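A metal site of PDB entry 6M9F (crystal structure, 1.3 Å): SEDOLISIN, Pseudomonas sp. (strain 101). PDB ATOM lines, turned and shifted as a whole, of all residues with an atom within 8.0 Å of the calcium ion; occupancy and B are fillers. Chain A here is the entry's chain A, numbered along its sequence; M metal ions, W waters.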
ATOM      1  N   VAL A 217      20.499 -11.867  33.335  1.00  0.00           N
ATOM      2  CA  VAL A 217      21.017 -10.546  33.716  1.00  0.00           C
ATOM      3  C   VAL A 217      20.556 -10.193  35.114  1.00  0.00           C
ATOM      4  O   VAL A 217      19.410 -10.440  35.474  1.00  0.00           O
ATOM      5  CB  VAL A 217      20.550  -9.476  32.714  1.00  0.00           C
ATOM      6  CG1 VAL A 217      21.005  -8.082  33.119  1.00  0.00           C
ATOM      7  CG2 VAL A 217      21.019  -9.736  31.292  1.00  0.00           C
ATOM      8  N   VAL A 324      32.684 -20.381  29.090  1.00  0.00           N
ATOM      9  CA  VAL A 324      31.770 -19.506  29.842  1.00  0.00           C
ATOM     10  C   VAL A 324      30.352 -20.064  29.869  1.00  0.00           C
ATOM     11  O   VAL A 324      29.951 -20.874  29.061  1.00  0.00           O
ATOM     12  CB  VAL A 324      31.734 -18.065  29.283  1.00  0.00           C
ATOM     13  CG1 VAL A 324      33.099 -17.433  29.542  1.00  0.00           C
ATOM     14  CG2 VAL A 324      31.314 -18.051  27.818  1.00  0.00           C
ATOM     15  N   HIS A 325      29.629 -19.540  30.876  1.00  0.00           N
ATOM     16  CA  HIS A 325      28.185 -19.587  30.890  1.00  0.00           C
ATOM     17  C   HIS A 325      27.697 -18.282  30.225  1.00  0.00           C
ATOM     18  O   HIS A 325      27.803 -17.224  30.814  1.00  0.00           O
ATOM     19  CB  HIS A 325      27.591 -19.701  32.277  1.00  0.00           C
ATOM     20  CG  HIS A 325      28.003 -20.902  33.040  1.00  0.00           C
ATOM     21  ND1 HIS A 325      27.574 -22.170  32.681  1.00  0.00           N
ATOM     22  CD2 HIS A 325      28.799 -21.056  34.093  1.00  0.00           C
ATOM     23  CE1 HIS A 325      28.095 -23.057  33.507  1.00  0.00           C
ATOM     24  NE2 HIS A 325      28.850 -22.402  34.384  1.00  0.00           N
ATOM     25  N   ASP A 326      27.199 -18.396  29.005  1.00  0.00           N
ATOM     26  CA  ASP A 326      26.756 -17.280  28.184  1.00  0.00           C
ATOM     27  C   ASP A 326      25.368 -16.825  28.661  1.00  0.00           C
ATOM     28  O   ASP A 326      24.372 -17.523  28.498  1.00  0.00           O
ATOM     29  CB  ASP A 326      26.702 -17.666  26.712  1.00  0.00           C
ATOM     30  CG  ASP A 326      26.306 -16.503  25.822  1.00  0.00           C
ATOM     31  OD1 ASP A 326      26.411 -15.329  26.255  1.00  0.00           O
ATOM     32  OD2 ASP A 326      25.954 -16.817  24.658  1.00  0.00           O
ATOM     33  N   VAL A 327      25.264 -15.631  29.209  1.00  0.00           N
ATOM     34  CA  VAL A 327      23.983 -15.057  29.617  1.00  0.00           C
ATOM     35  C   VAL A 327      23.288 -14.523  28.368  1.00  0.00           C
ATOM     36  O   VAL A 327      23.894 -13.818  27.581  1.00  0.00           O
ATOM     37  CB  VAL A 327      24.172 -13.960  30.666  1.00  0.00           C
ATOM     38  CG1 VAL A 327      22.819 -13.344  31.019  1.00  0.00           C
ATOM     39  CG2 VAL A 327      24.860 -14.540  31.880  1.00  0.00           C
ATOM     40  N   LYS A 328      21.999 -14.898  28.251  1.00  0.00           N
ATOM     41  CA  LYS A 328      21.227 -14.588  27.064  1.00  0.00           C
ATOM     42  C   LYS A 328      19.951 -13.845  27.383  1.00  0.00           C
ATOM     43  O   LYS A 328      19.416 -13.222  26.437  1.00  0.00           O
ATOM     44  CB  LYS A 328      20.915 -15.855  26.269  1.00  0.00           C
ATOM     45  CG  LYS A 328      22.157 -16.511  25.647  1.00  0.00           C
ATOM     46  CD  LYS A 328      21.703 -17.778  24.905  1.00  0.00           C
ATOM     47  CE  LYS A 328      22.887 -18.644  24.542  1.00  0.00           C
ATOM     48  NZ  LYS A 328      22.436 -19.734  23.636  1.00  0.00           N
ATOM     49  N   SER A 329      19.457 -13.845  28.621  1.00  0.00           N
ATOM     50  CA  SER A 329      18.162 -13.269  28.907  1.00  0.00           C
ATOM     51  C   SER A 329      18.233 -12.108  29.887  1.00  0.00           C
ATOM     52  O   SER A 329      18.863 -12.262  30.926  1.00  0.00           O
ATOM     53  CB  SER A 329      17.222 -14.346  29.479  1.00  0.00           C
ATOM     54  OG  SER A 329      16.079 -13.803  30.085  1.00  0.00           O
ATOM     55  N   ASN A 340      20.221  -5.182  26.021  1.00  0.00           N
ATOM     56  CA  ASN A 340      19.739  -6.558  26.102  1.00  0.00           C
ATOM     57  C   ASN A 340      20.863  -7.554  26.084  1.00  0.00           C
ATOM     58  O   ASN A 340      21.784  -7.461  25.284  1.00  0.00           O
ATOM     59  CB  ASN A 340      18.814  -6.852  24.924  1.00  0.00           C
ATOM     60  CG  ASN A 340      17.624  -5.895  24.943  1.00  0.00           C
ATOM     61  OD1 ASN A 340      16.958  -5.788  25.968  1.00  0.00           O
ATOM     62  ND2 ASN A 340      17.418  -5.222  23.831  1.00  0.00           N
ATOM     63  N   ALA A 341      20.778  -8.601  26.913  1.00  0.00           N
ATOM     64  CA  ALA A 341      21.646  -9.749  26.738  1.00  0.00           C
ATOM     65  C   ALA A 341      21.336 -10.474  25.431  1.00  0.00           C
ATOM     66  O   ALA A 341      20.297 -10.348  24.815  1.00  0.00           O
ATOM     67  CB  ALA A 341      21.518 -10.677  27.947  1.00  0.00           C
ATOM     68  N   GLY A 342      22.296 -11.252  24.957  1.00  0.00           N
ATOM     69  CA  GLY A 342      22.165 -12.055  23.756  1.00  0.00           C
ATOM     70  C   GLY A 342      23.309 -13.038  23.655  1.00  0.00           C
ATOM     71  O   GLY A 342      24.134 -13.253  24.538  1.00  0.00           O
ATOM     72  N   THR A 343      23.334 -13.704  22.496  1.00  0.00           N
ATOM     73  CA  THR A 343      24.382 -14.700  22.258  1.00  0.00           C
ATOM     74  C   THR A 343      25.738 -14.032  22.249  1.00  0.00           C
ATOM     75  O   THR A 343      25.922 -12.987  21.602  1.00  0.00           O
ATOM     76  CB  THR A 343      24.088 -15.407  20.922  1.00  0.00           C
ATOM     77  OG1 THR A 343      22.897 -16.167  21.087  1.00  0.00           O
ATOM     78  CG2 THR A 343      25.197 -16.391  20.578  1.00  0.00           C
ATOM     79  N   GLY A 344      26.686 -14.609  22.975  1.00  0.00           N
ATOM     80  CA  GLY A 344      28.022 -14.102  23.046  1.00  0.00           C
ATOM     81  C   GLY A 344      28.133 -12.857  23.922  1.00  0.00           C
ATOM     82  O   GLY A 344      27.352 -12.629  24.849  1.00  0.00           O
ATOM     83  N   TRP A 345      29.117 -12.021  23.609  1.00  0.00           N
ATOM     84  CA  TRP A 345      29.364 -10.833  24.404  1.00  0.00           C
ATOM     85  C   TRP A 345      28.181  -9.896  24.330  1.00  0.00           C
ATOM     86  O   TRP A 345      27.699  -9.615  23.231  1.00  0.00           O
ATOM     87  CB  TRP A 345      30.674 -10.138  23.945  1.00  0.00           C
ATOM     88  CG  TRP A 345      31.143  -9.086  24.912  1.00  0.00           C
ATOM     89  CD1 TRP A 345      32.146  -9.249  25.842  1.00  0.00           C
ATOM     90  CD2 TRP A 345      30.676  -7.747  25.054  1.00  0.00           C
ATOM     91  NE1 TRP A 345      32.300  -8.100  26.513  1.00  0.00           N
ATOM     92  CE2 TRP A 345      31.416  -7.157  26.079  1.00  0.00           C
ATOM     93  CE3 TRP A 345      29.682  -6.974  24.409  1.00  0.00           C
ATOM     94  CZ2 TRP A 345      31.213  -5.853  26.492  1.00  0.00           C
ATOM     95  CZ3 TRP A 345      29.493  -5.679  24.832  1.00  0.00           C
ATOM     96  CH2 TRP A 345      30.253  -5.116  25.865  1.00  0.00           C
ATOM     97  N   ASP A 346      27.740  -9.338  25.437  1.00  0.00           N
ATOM     98  CA  ASP A 346      26.712  -8.313  25.420  1.00  0.00           C
ATOM     99  C   ASP A 346      27.008  -7.228  26.459  1.00  0.00           C
ATOM    100  O   ASP A 346      27.845  -7.399  27.346  1.00  0.00           O
ATOM    101  CB  ASP A 346      25.338  -8.962  25.625  1.00  0.00           C
ATOM    102  CG  ASP A 346      25.164  -9.831  26.859  1.00  0.00           C
ATOM    103  OD1 ASP A 346      25.386  -9.290  27.969  1.00  0.00           O
ATOM    104  OD2 ASP A 346      24.838 -11.031  26.704  1.00  0.00           O
ATOM    105  N   TYR A 347      26.309  -6.108  26.382  1.00  0.00           N
ATOM    106  CA  TYR A 347      26.620  -4.999  27.273  1.00  0.00           C
ATOM    107  C   TYR A 347      26.199  -5.265  28.722  1.00  0.00           C
ATOM    108  O   TYR A 347      26.909  -4.758  29.606  1.00  0.00           O
ATOM    109  CB  TYR A 347      25.994  -3.713  26.741  1.00  0.00           C
ATOM    110  CG  TYR A 347      26.687  -3.104  25.552  1.00  0.00           C
ATOM    111  CD1 TYR A 347      26.141  -3.124  24.291  1.00  0.00           C
ATOM    112  CD2 TYR A 347      27.936  -2.515  25.694  1.00  0.00           C
ATOM    113  CE1 TYR A 347      26.790  -2.570  23.199  1.00  0.00           C
ATOM    114  CE2 TYR A 347      28.608  -1.947  24.625  1.00  0.00           C
ATOM    115  CZ  TYR A 347      28.030  -1.975  23.383  1.00  0.00           C
ATOM    116  OH  TYR A 347      28.692  -1.406  22.287  1.00  0.00           O
ATOM    117  N   PRO A 348      25.122  -5.968  29.042  1.00  0.00           N
ATOM    118  CA  PRO A 348      24.846  -6.193  30.452  1.00  0.00           C
ATOM    119  C   PRO A 348      25.860  -7.048  31.194  1.00  0.00           C
ATOM    120  O   PRO A 348      26.149  -6.826  32.365  1.00  0.00           O
ATOM    121  CB  PRO A 348      23.466  -6.875  30.485  1.00  0.00           C
ATOM    122  CG  PRO A 348      22.820  -6.251  29.271  1.00  0.00           C
ATOM    123  CD  PRO A 348      23.945  -6.383  28.241  1.00  0.00           C
ATOM    124  N   THR A 349      26.389  -8.066  30.499  1.00  0.00           N
ATOM    125  CA  THR A 349      27.117  -9.125  31.185  1.00  0.00           C
ATOM    126  C   THR A 349      28.459  -9.488  30.576  1.00  0.00           C
ATOM    127  O   THR A 349      29.199 -10.339  31.095  1.00  0.00           O
ATOM    128  CB  THR A 349      26.294 -10.446  31.348  1.00  0.00           C
ATOM    129  OG1 THR A 349      25.958 -10.966  30.076  1.00  0.00           O
ATOM    130  CG2 THR A 349      25.026 -10.137  32.124  1.00  0.00           C
ATOM    131  N   GLY A 350      28.863  -8.867  29.471  1.00  0.00           N
ATOM    132  CA  GLY A 350      30.108  -9.196  28.838  1.00  0.00           C
ATOM    133  C   GLY A 350      30.046 -10.606  28.311  1.00  0.00           C
ATOM    134  O   GLY A 350      29.033 -10.992  27.707  1.00  0.00           O
ATOM    135  N   TRP A 351      31.088 -11.421  28.582  1.00  0.00           N
ATOM    136  CA  TRP A 351      31.113 -12.798  28.144  1.00  0.00           C
ATOM    137  C   TRP A 351      30.287 -13.736  29.015  1.00  0.00           C
ATOM    138  O   TRP A 351      30.138 -14.903  28.659  1.00  0.00           O
ATOM    139  CB  TRP A 351      32.558 -13.302  28.120  1.00  0.00           C
ATOM    140  CG  TRP A 351      33.394 -12.722  27.058  1.00  0.00           C
ATOM    141  CD1 TRP A 351      34.467 -11.908  27.240  1.00  0.00           C
ATOM    142  CD2 TRP A 351      33.235 -12.873  25.629  1.00  0.00           C
ATOM    143  NE1 TRP A 351      35.005 -11.555  26.013  1.00  0.00           N
ATOM    144  CE2 TRP A 351      34.273 -12.132  25.008  1.00  0.00           C
ATOM    145  CE3 TRP A 351      32.366 -13.544  24.786  1.00  0.00           C
ATOM    146  CZ2 TRP A 351      34.412 -12.064  23.630  1.00  0.00           C
ATOM    147  CZ3 TRP A 351      32.487 -13.498  23.415  1.00  0.00           C
ATOM    148  CH2 TRP A 351      33.529 -12.748  22.837  1.00  0.00           C
ATOM    149  N   GLY A 352      29.799 -13.263  30.154  1.00  0.00           N
ATOM    150  CA  GLY A 352      29.103 -14.086  31.152  1.00  0.00           C
ATOM    151  C   GLY A 352      30.086 -14.585  32.198  1.00  0.00           C
ATOM    152  O   GLY A 352      31.130 -13.973  32.432  1.00  0.00           O
HETATM  153 CA    CA M   1      25.633 -13.146  26.300  1.00  0.00          CA
HETATM  154  O   HOH W   1      27.024 -12.846  28.278  1.00  0.00           O
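The side-chain carboxylate of Asp 346 lies within hydrogen-bond range of the side-chain hydroxyl of Thr 349, at 2.8 Å.
Within 4 Å of the calcium ion: Asp 326, Val 327, Gly 342, Gly 344 and Asp 346. The nearest printed residue that does not touch the calcium ion is Thr 343 (4.1 Å).
The calcium ion is bound by O of Val 327 (2.3 Å), OD2 of Asp 346 (2.3 Å), O of Gly 344 (2.3 Å), O of Gly 342 (2.3 Å), OD1 of Asp 326 (2.3 Å) and water W1 (2.4 Å).
Water W1 lies within hydrogen-bond range of O of Gly 350, OG1 of Thr 349, N of Gly 352 and N of Val 327.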
